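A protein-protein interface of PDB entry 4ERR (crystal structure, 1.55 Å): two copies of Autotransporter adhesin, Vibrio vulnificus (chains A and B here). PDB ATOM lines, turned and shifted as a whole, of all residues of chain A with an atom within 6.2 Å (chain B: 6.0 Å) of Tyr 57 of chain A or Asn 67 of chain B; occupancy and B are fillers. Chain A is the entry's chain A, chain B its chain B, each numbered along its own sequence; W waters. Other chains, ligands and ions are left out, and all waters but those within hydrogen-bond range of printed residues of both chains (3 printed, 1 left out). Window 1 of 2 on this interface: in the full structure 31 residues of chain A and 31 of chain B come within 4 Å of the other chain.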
ATOM      1  N   ILE A  21      -4.329  13.340   9.225  1.00  0.00           N
ATOM      2  CA  ILE A  21      -5.126  14.292  10.006  1.00  0.00           C
ATOM      3  C   ILE A  21      -4.158  15.219  10.748  1.00  0.00           C
ATOM      4  O   ILE A  21      -4.315  16.428  10.759  1.00  0.00           O
ATOM      5  CB  ILE A  21      -6.062  13.577  11.020  1.00  0.00           C
ATOM      6  CG1 ILE A  21      -6.977  12.569  10.305  1.00  0.00           C
ATOM      7  CG2 ILE A  21      -6.917  14.582  11.784  1.00  0.00           C
ATOM      8  CD1 ILE A  21      -7.850  11.742  11.235  1.00  0.00           C
ATOM      9  N   GLY A  22      -3.129  14.649  11.343  1.00  0.00           N
ATOM     10  CA  GLY A  22      -2.143  15.461  12.026  1.00  0.00           C
ATOM     11  C   GLY A  22      -1.396  16.443  11.129  1.00  0.00           C
ATOM     12  O   GLY A  22      -1.090  17.570  11.544  1.00  0.00           O
ATOM     13  N   SER A  24      -2.615  17.851   8.421  1.00  0.00           N
ATOM     14  CA  SER A  24      -3.579  18.956   8.197  1.00  0.00           C
ATOM     15  C   SER A  24      -3.680  19.887   9.418  1.00  0.00           C
ATOM     16  O   SER A  24      -3.701  21.107   9.298  1.00  0.00           O
ATOM     17  CB  SER A  24      -4.979  18.426   7.844  1.00  0.00           C
ATOM     18  OG  SER A  24      -5.005  17.773   6.581  1.00  0.00           O
ATOM     19  N   TYR A  25      -3.743  19.299  10.604  1.00  0.00           N
ATOM     20  CA  TYR A  25      -3.820  20.090  11.822  1.00  0.00           C
ATOM     21  C   TYR A  25      -2.601  20.994  11.963  1.00  0.00           C
ATOM     22  O   TYR A  25      -2.762  22.138  12.316  1.00  0.00           O
ATOM     23  CB  TYR A  25      -3.934  19.171  13.012  1.00  0.00           C
ATOM     24  CG  TYR A  25      -4.077  19.832  14.355  1.00  0.00           C
ATOM     25  CD1 TYR A  25      -5.134  20.679  14.619  1.00  0.00           C
ATOM     26  CD2 TYR A  25      -3.160  19.595  15.370  1.00  0.00           C
ATOM     27  CE1 TYR A  25      -5.290  21.271  15.875  1.00  0.00           C
ATOM     28  CE2 TYR A  25      -3.303  20.172  16.627  1.00  0.00           C
ATOM     29  CZ  TYR A  25      -4.374  21.020  16.866  1.00  0.00           C
ATOM     30  OH  TYR A  25      -4.562  21.599  18.096  1.00  0.00           O
ATOM     31  N   ILE A  28      -3.032  24.172  10.152  1.00  0.00           N
ATOM     32  CA  ILE A  28      -3.899  25.088  10.875  1.00  0.00           C
ATOM     33  C   ILE A  28      -3.118  25.847  11.941  1.00  0.00           C
ATOM     34  O   ILE A  28      -3.238  27.078  12.056  1.00  0.00           O
ATOM     35  CB  ILE A  28      -5.133  24.368  11.497  1.00  0.00           C
ATOM     36  CG1 ILE A  28      -6.068  23.909  10.377  1.00  0.00           C
ATOM     37  CG2 ILE A  28      -5.882  25.299  12.435  1.00  0.00           C
ATOM     38  CD1 ILE A  28      -7.168  22.979  10.887  1.00  0.00           C
ATOM     39  N   LYS A  52     -10.644  29.122   5.917  1.00  0.00           N
ATOM     40  CA  LYS A  52     -10.700  28.088   4.877  1.00  0.00           C
ATOM     41  C   LYS A  52      -9.991  26.809   5.330  1.00  0.00           C
ATOM     42  O   LYS A  52     -10.525  25.713   5.155  1.00  0.00           O
ATOM     43  CB  LYS A  52     -10.099  28.598   3.573  1.00  0.00           C
ATOM     44  CG  LYS A  52     -10.080  27.549   2.479  1.00  0.00           C
ATOM     45  CD  LYS A  52      -9.491  28.068   1.183  1.00  0.00           C
ATOM     46  CE  LYS A  52      -9.300  26.963   0.174  1.00  0.00           C
ATOM     47  NZ  LYS A  52      -8.364  25.903   0.687  1.00  0.00           N
ATOM     48  N   LYS A  53      -8.801  26.934   5.923  1.00  0.00           N
ATOM     49  CA  LYS A  53      -8.082  25.747   6.398  1.00  0.00           C
ATOM     50  C   LYS A  53      -8.897  24.946   7.414  1.00  0.00           C
ATOM     51  O   LYS A  53      -8.896  23.711   7.380  1.00  0.00           O
ATOM     52  CB  LYS A  53      -6.704  26.092   6.926  1.00  0.00           C
ATOM     53  CG  LYS A  53      -5.702  26.524   5.857  1.00  0.00           C
ATOM     54  CD  LYS A  53      -4.342  26.880   6.455  1.00  0.00           C
ATOM     55  CE  LYS A  53      -3.389  27.437   5.399  1.00  0.00           C
ATOM     56  NZ  LYS A  53      -3.100  26.400   4.431  1.00  0.00           N
ATOM     57  N   ILE A  54      -9.589  25.631   8.312  1.00  0.00           N
ATOM     58  CA  ILE A  54     -10.419  24.932   9.295  1.00  0.00           C
ATOM     59  C   ILE A  54     -11.578  24.248   8.602  1.00  0.00           C
ATOM     60  O   ILE A  54     -11.854  23.080   8.858  1.00  0.00           O
ATOM     61  CB  ILE A  54     -10.900  25.833  10.433  1.00  0.00           C
ATOM     62  CG1 ILE A  54      -9.714  26.452  11.190  1.00  0.00           C
ATOM     63  CG2 ILE A  54     -11.773  25.031  11.406  1.00  0.00           C
ATOM     64  CD1 ILE A  54     -10.109  27.589  12.138  1.00  0.00           C
ATOM     65  N   ASN A  55     -12.250  24.973   7.714  1.00  0.00           N
ATOM     66  CA  ASN A  55     -13.349  24.398   6.978  1.00  0.00           C
ATOM     67  C   ASN A  55     -12.920  23.124   6.263  1.00  0.00           C
ATOM     68  O   ASN A  55     -13.582  22.083   6.389  1.00  0.00           O
ATOM     69  CB  ASN A  55     -13.892  25.377   5.950  1.00  0.00           C
ATOM     70  CG  ASN A  55     -14.939  24.751   5.099  1.00  0.00           C
ATOM     71  OD1 ASN A  55     -14.655  24.253   3.996  1.00  0.00           O
ATOM     72  ND2 ASN A  55     -16.149  24.682   5.629  1.00  0.00           N
ATOM     73  N   ASP A  56     -11.796  23.207   5.547  1.00  0.00           N
ATOM     74  CA  ASP A  56     -11.266  22.093   4.761  1.00  0.00           C
ATOM     75  C   ASP A  56     -10.908  20.895   5.653  1.00  0.00           C
ATOM     76  O   ASP A  56     -11.166  19.742   5.301  1.00  0.00           O
ATOM     77  CB  ASP A  56     -10.024  22.546   3.980  1.00  0.00           C
ATOM     78  CG  ASP A  56     -10.334  23.547   2.876  1.00  0.00           C
ATOM     79  OD1 ASP A  56     -11.495  23.752   2.494  1.00  0.00           O
ATOM     80  OD2 ASP A  56      -9.377  24.131   2.380  1.00  0.00           O
ATOM     81  N   TYR A  57     -10.334  21.180   6.822  1.00  0.00           N
ATOM     82  CA  TYR A  57      -9.963  20.142   7.774  1.00  0.00           C
ATOM     83  C   TYR A  57     -11.217  19.407   8.273  1.00  0.00           C
ATOM     84  O   TYR A  57     -11.254  18.178   8.318  1.00  0.00           O
ATOM     85  CB  TYR A  57      -9.156  20.745   8.944  1.00  0.00           C
ATOM     86  CG  TYR A  57      -8.922  19.783  10.103  1.00  0.00           C
ATOM     87  CD1 TYR A  57      -9.923  19.536  11.018  1.00  0.00           C
ATOM     88  CD2 TYR A  57      -7.707  19.104  10.263  1.00  0.00           C
ATOM     89  CE1 TYR A  57      -9.746  18.639  12.069  1.00  0.00           C
ATOM     90  CE2 TYR A  57      -7.517  18.221  11.331  1.00  0.00           C
ATOM     91  CZ  TYR A  57      -8.548  17.990  12.213  1.00  0.00           C
ATOM     92  OH  TYR A  57      -8.351  17.100  13.260  1.00  0.00           O
ATOM     93  N   ILE A  58     -12.244  20.164   8.648  1.00  0.00           N
ATOM     94  CA  ILE A  58     -13.447  19.597   9.241  1.00  0.00           C
ATOM     95  C   ILE A  58     -14.147  18.743   8.222  1.00  0.00           C
ATOM     96  O   ILE A  58     -14.746  17.694   8.577  1.00  0.00           O
ATOM     97  CB  ILE A  58     -14.376  20.692   9.859  1.00  0.00           C
ATOM     98  CG1 ILE A  58     -13.687  21.331  11.053  1.00  0.00           C
ATOM     99  CG2 ILE A  58     -15.723  20.089  10.309  1.00  0.00           C
ATOM    100  CD1 ILE A  58     -14.477  22.412  11.718  1.00  0.00           C
ATOM    101  N   ALA A  59     -14.052  19.144   6.957  1.00  0.00           N
ATOM    102  CA  ALA A  59     -14.692  18.406   5.887  1.00  0.00           C
ATOM    103  C   ALA A  59     -13.970  17.107   5.561  1.00  0.00           C
ATOM    104  O   ALA A  59     -14.619  16.075   5.269  1.00  0.00           O
ATOM    105  CB  ALA A  59     -14.787  19.265   4.639  1.00  0.00           C
ATOM    106  N   GLU A  60     -12.637  17.148   5.586  1.00  0.00           N
ATOM    107  CA  GLU A  60     -11.808  16.001   5.199  1.00  0.00           C
ATOM    108  C   GLU A  60     -11.514  15.058   6.362  1.00  0.00           C
ATOM    109  O   GLU A  60     -11.274  13.872   6.137  1.00  0.00           O
ATOM    110  CB  GLU A  60     -10.504  16.486   4.541  1.00  0.00           C
ATOM    111  CG  GLU A  60      -9.367  15.445   4.425  1.00  0.00           C
ATOM    112  CD  GLU A  60      -9.599  14.321   3.397  1.00  0.00           C
ATOM    113  OE1 GLU A  60     -10.401  13.393   3.654  1.00  0.00           O
ATOM    114  OE2 GLU A  60      -8.915  14.330   2.352  1.00  0.00           O
ATOM    115  N   HIS A  61     -11.552  15.565   7.593  1.00  0.00           N
ATOM    116  CA  HIS A  61     -11.210  14.759   8.773  1.00  0.00           C
ATOM    117  C   HIS A  61     -12.228  14.809   9.941  1.00  0.00           C
ATOM    118  O   HIS A  61     -11.880  15.131  11.073  1.00  0.00           O
ATOM    119  CB  HIS A  61      -9.810  15.195   9.292  1.00  0.00           C
ATOM    120  CG  HIS A  61      -8.746  15.285   8.233  1.00  0.00           C
ATOM    121  ND1 HIS A  61      -8.323  14.204   7.501  1.00  0.00           N
ATOM    122  CD2 HIS A  61      -7.976  16.332   7.831  1.00  0.00           C
ATOM    123  CE1 HIS A  61      -7.351  14.576   6.682  1.00  0.00           C
ATOM    124  NE2 HIS A  61      -7.137  15.873   6.852  1.00  0.00           N
ATOM    125  N   PRO A  62     -13.464  14.358   9.699  1.00  0.00           N
ATOM    126  CA  PRO A  62     -14.496  14.342  10.746  1.00  0.00           C
ATOM    127  C   PRO A  62     -14.309  13.295  11.829  1.00  0.00           C
ATOM    128  O   PRO A  62     -14.859  13.430  12.949  1.00  0.00           O
ATOM    129  CB  PRO A  62     -15.774  14.040   9.954  1.00  0.00           C
ATOM    130  CG  PRO A  62     -15.310  13.228   8.765  1.00  0.00           C
ATOM    131  CD  PRO A  62     -13.942  13.802   8.427  1.00  0.00           C
ATOM    132  N   THR A  63     -13.528  12.258  11.543  1.00  0.00           N
ATOM    133  CA  THR A  63     -13.396  11.148  12.478  1.00  0.00           C
ATOM    134  C   THR A  63     -11.935  10.889  12.760  1.00  0.00           C
ATOM    135  O   THR A  63     -11.126  10.718  11.842  1.00  0.00           O
ATOM    136  CB  THR A  63     -14.062   9.901  11.914  1.00  0.00           C
ATOM    137  OG1 THR A  63     -15.448  10.189  11.660  1.00  0.00           O
ATOM    138  CG2 THR A  63     -13.957   8.696  12.901  1.00  0.00           C
ATOM    139  N   SER A  64     -11.593  10.840  14.043  1.00  0.00           N
ATOM    140  CA  SER A  64     -10.212  10.692  14.424  1.00  0.00           C
ATOM    141  C   SER A  64      -9.641   9.346  13.958  1.00  0.00           C
ATOM    142  O   SER A  64     -10.372   8.405  13.699  1.00  0.00           O
ATOM    143  CB  SER A  64     -10.095  10.818  15.947  1.00  0.00           C
ATOM    144  OG  SER A  64     -10.717   9.705  16.562  1.00  0.00           O
ATOM    145  N   THR B  63     -16.551  13.075  18.691  1.00  0.00           N
ATOM    146  CA  THR B  63     -15.706  14.130  18.196  1.00  0.00           C
ATOM    147  C   THR B  63     -14.485  14.301  19.119  1.00  0.00           C
ATOM    148  O   THR B  63     -14.620  14.454  20.360  1.00  0.00           O
ATOM    149  CB  THR B  63     -16.509  15.436  18.126  1.00  0.00           C
ATOM    150  OG1 THR B  63     -17.679  15.187  17.348  1.00  0.00           O
ATOM    151  CG2 THR B  63     -15.703  16.577  17.500  1.00  0.00           C
ATOM    152  N   SER B  64     -13.307  14.270  18.507  1.00  0.00           N
ATOM    153  CA  SER B  64     -12.057  14.343  19.249  1.00  0.00           C
ATOM    154  C   SER B  64     -11.941  15.666  20.007  1.00  0.00           C
ATOM    155  O   SER B  64     -12.590  16.672  19.677  1.00  0.00           O
ATOM    156  CB  SER B  64     -10.865  14.199  18.305  1.00  0.00           C
ATOM    157  OG  SER B  64     -10.735  15.326  17.465  1.00  0.00           O
ATOM    158  N   GLY B  65     -11.101  15.687  21.022  1.00  0.00           N
ATOM    159  CA  GLY B  65     -10.801  16.946  21.734  1.00  0.00           C
ATOM    160  C   GLY B  65     -10.322  18.044  20.785  1.00  0.00           C
ATOM    161  O   GLY B  65     -10.756  19.183  20.851  1.00  0.00           O
ATOM    162  N   ARG B  66      -9.396  17.689  19.905  1.00  0.00           N
ATOM    163  CA  ARG B  66      -8.901  18.591  18.899  1.00  0.00           C
ATOM    164  C   ARG B  66     -10.041  19.150  18.048  1.00  0.00           C
ATOM    165  O   ARG B  66     -10.152  20.362  17.834  1.00  0.00           O
ATOM    166  CB  ARG B  66      -7.944  17.821  18.001  1.00  0.00           C
ATOM    167  CG  ARG B  66      -7.459  18.608  16.859  1.00  0.00           C
ATOM    168  CD  ARG B  66      -6.689  17.722  15.897  1.00  0.00           C
ATOM    169  NE  ARG B  66      -5.499  17.150  16.496  1.00  0.00           N
ATOM    170  CZ  ARG B  66      -4.733  16.233  15.901  1.00  0.00           C
ATOM    171  NH1 ARG B  66      -5.059  15.759  14.707  1.00  0.00           N
ATOM    172  NH2 ARG B  66      -3.645  15.778  16.505  1.00  0.00           N
ATOM    173  N   ASN B  67     -10.908  18.278  17.562  1.00  0.00           N
ATOM    174  CA  ASN B  67     -11.976  18.750  16.680  1.00  0.00           C
ATOM    175  C   ASN B  67     -12.962  19.657  17.400  1.00  0.00           C
ATOM    176  O   ASN B  67     -13.436  20.642  16.831  1.00  0.00           O
ATOM    177  CB  ASN B  67     -12.663  17.604  15.931  1.00  0.00           C
ATOM    178  CG  ASN B  67     -11.850  17.112  14.734  1.00  0.00           C
ATOM    179  OD1 ASN B  67     -10.607  17.089  14.779  1.00  0.00           O
ATOM    180  ND2 ASN B  67     -12.537  16.756  13.654  1.00  0.00           N
ATOM    181  N   GLN B  68     -13.259  19.326  18.651  1.00  0.00           N
ATOM    182  CA  GLN B  68     -14.121  20.181  19.462  1.00  0.00           C
ATOM    183  C   GLN B  68     -13.501  21.565  19.618  1.00  0.00           C
ATOM    184  O   GLN B  68     -14.212  22.574  19.483  1.00  0.00           O
ATOM    185  CB  GLN B  68     -14.389  19.579  20.832  1.00  0.00           C
ATOM    186  CG  GLN B  68     -15.281  18.365  20.853  1.00  0.00           C
ATOM    187  CD  GLN B  68     -15.413  17.797  22.242  1.00  0.00           C
ATOM    188  OE1 GLN B  68     -14.879  16.713  22.547  1.00  0.00           O
ATOM    189  NE2 GLN B  68     -16.069  18.523  23.094  1.00  0.00           N
ATOM    190  N   ALA B  69     -12.196  21.631  19.872  1.00  0.00           N
ATOM    191  CA  ALA B  69     -11.499  22.924  20.035  1.00  0.00           C
ATOM    192  C   ALA B  69     -11.447  23.700  18.711  1.00  0.00           C
ATOM    193  O   ALA B  69     -11.633  24.920  18.675  1.00  0.00           O
ATOM    194  CB  ALA B  69     -10.071  22.713  20.601  1.00  0.00           C
ATOM    195  N   LEU B  70     -11.181  22.990  17.624  1.00  0.00           N
ATOM    196  CA  LEU B  70     -11.187  23.619  16.286  1.00  0.00           C
ATOM    197  C   LEU B  70     -12.569  24.199  15.906  1.00  0.00           C
ATOM    198  O   LEU B  70     -12.645  25.218  15.229  1.00  0.00           O
ATOM    199  CB  LEU B  70     -10.719  22.635  15.226  1.00  0.00           C
ATOM    200  CG  LEU B  70      -9.233  22.305  15.205  1.00  0.00           C
ATOM    201  CD1 LEU B  70      -8.956  21.198  14.202  1.00  0.00           C
ATOM    202  CD2 LEU B  70      -8.411  23.542  14.902  1.00  0.00           C
ATOM    203  N   THR B  71     -13.644  23.528  16.308  1.00  0.00           N
ATOM    204  CA  THR B  71     -14.991  24.019  16.052  1.00  0.00           C
ATOM    205  C   THR B  71     -15.189  25.349  16.786  1.00  0.00           C
ATOM    206  O   THR B  71     -15.789  26.260  16.239  1.00  0.00           O
ATOM    207  CB  THR B  71     -16.053  22.961  16.389  1.00  0.00           C
ATOM    208  OG1 THR B  71     -15.884  21.842  15.502  1.00  0.00           O
ATOM    209  CG2 THR B  71     -17.494  23.507  16.273  1.00  0.00           C
ATOM    210  N   GLN B  72     -14.662  25.449  18.016  1.00  0.00           N
ATOM    211  CA  GLN B  72     -14.738  26.713  18.753  1.00  0.00           C
ATOM    212  C   GLN B  72     -13.880  27.790  18.090  1.00  0.00           C
ATOM    213  O   GLN B  72     -14.300  28.953  17.977  1.00  0.00           O
ATOM    214  CB  GLN B  72     -14.372  26.501  20.227  1.00  0.00           C
ATOM    215  CG  GLN B  72     -15.389  25.623  20.939  1.00  0.00           C
ATOM    216  CD  GLN B  72     -15.113  25.453  22.422  1.00  0.00           C
ATOM    217  OE1 GLN B  72     -13.968  25.325  22.847  1.00  0.00           O
ATOM    218  NE2 GLN B  72     -16.168  25.488  23.217  1.00  0.00           N
HETATM  219  O   HOH W   1     -10.997  13.808  13.629  1.00  0.00           O
HETATM  220  O   HOH W   2      -4.030  13.151  14.327  1.00  0.00           O
HETATM  221  O   HOH W   3     -16.455  14.953  14.344  1.00  0.00           O
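2 positions are printed for both chains.
Of the 10 pairs that touch across the chains among the printed residues, none has its exchanged pair printed and touching as well.
Printed residues of chain A that touch a printed residue of chain B: Ile 21, Gly 22, Tyr 25, Ile 28, Ile 54, Tyr 57 and His 61.
Hydrophobic or aromatic side chains of chain A within 4 Å of the printed part of chain B: Ile 21, Tyr 25, Ile 28, Ile 54 and Tyr 57.
Among the printed residues, 10 pairs touch across the chains.
Among the printed residues, no Asp or Glu carboxylate lies within 4 Å of a Lys or Arg side-chain nitrogen of the other chain.
Among the printed residues, pairs that only touch across the chains: Ile 21 of chain A with Arg 66 of chain B (3.7 Å), Gly 22 of chain A with Arg 66 of chain B (3.97 Å), Tyr 25 of chain A with Arg 66 of chain B (3.6 Å), Tyr 25 of chain A with Leu 70 of chain B (3.9 Å), Ile 28 of chain A with Leu 70 of chain B (3.9 Å), Ile 54 of chain A with Leu 70 of chain B (3.9 Å), Tyr 57 of chain A with Arg 66 of chain B (3.2 Å) and Tyr 57 of chain A with Leu 70 of chain B (3.4 Å).
Water W3 bridges O of Pro 62 of chain A (2.6 Å) and OG1 of Thr 63 of chain B (3.3 Å).
Water W2 bridges NH1 of Arg 66 of chain B (2.8 Å) and N of Gly 22 of chain A (3.5 Å).
Water W1 lies within hydrogen-bond range of O of His 61 of chain A (3.0 Å), N of Ser 64 of chain A (3.1 Å) and ND2 of Asn 67 of chain B (3.3 Å).
The backbone carbonyl oxygen of Asn 67 of chain B lies within hydrogen-bond range of the side-chain hydroxyl of Thr 71 of chain B (3.0 Å).
OG of Ser 64 of chain B is in hydrogen-bond range of N of Asn 67 of chain B (3.0 Å).
The side-chain hydroxyl of Ser 24 of chain A sits at hydrogen-bond distance from a ring nitrogen (NE2) of His 61 of chain A, 2.9 Å away.
Of the printed residues of chain B, Gly 22 of chain A touches Arg 66 (3.97 Å).
Tyr 57 of chain A touches just these residues of chain B: Arg 66, Asn 67 and Leu 70.
Glu 60 of chain A touches none of the printed residues of chain B.
Of the printed residues of chain A, Arg 66 of chain B touches Ile 21, Gly 22, Tyr 25 and Tyr 57.
Asn 67 of chain B touches two residues of chain A.
The nearest residue of chain A that does not touch Asn 67 of chain B is Pro 62 of chain A (4.1 Å).
The side-chain hydroxyl (OH) of Tyr 57 of chain A lies within hydrogen-bond range of the side-chain amide oxygen (OD1) of Asn 67 of chain B.
ND2 of Asn 67 of chain B is in hydrogen-bond range of O of His 61 of chain A (3.1 Å).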
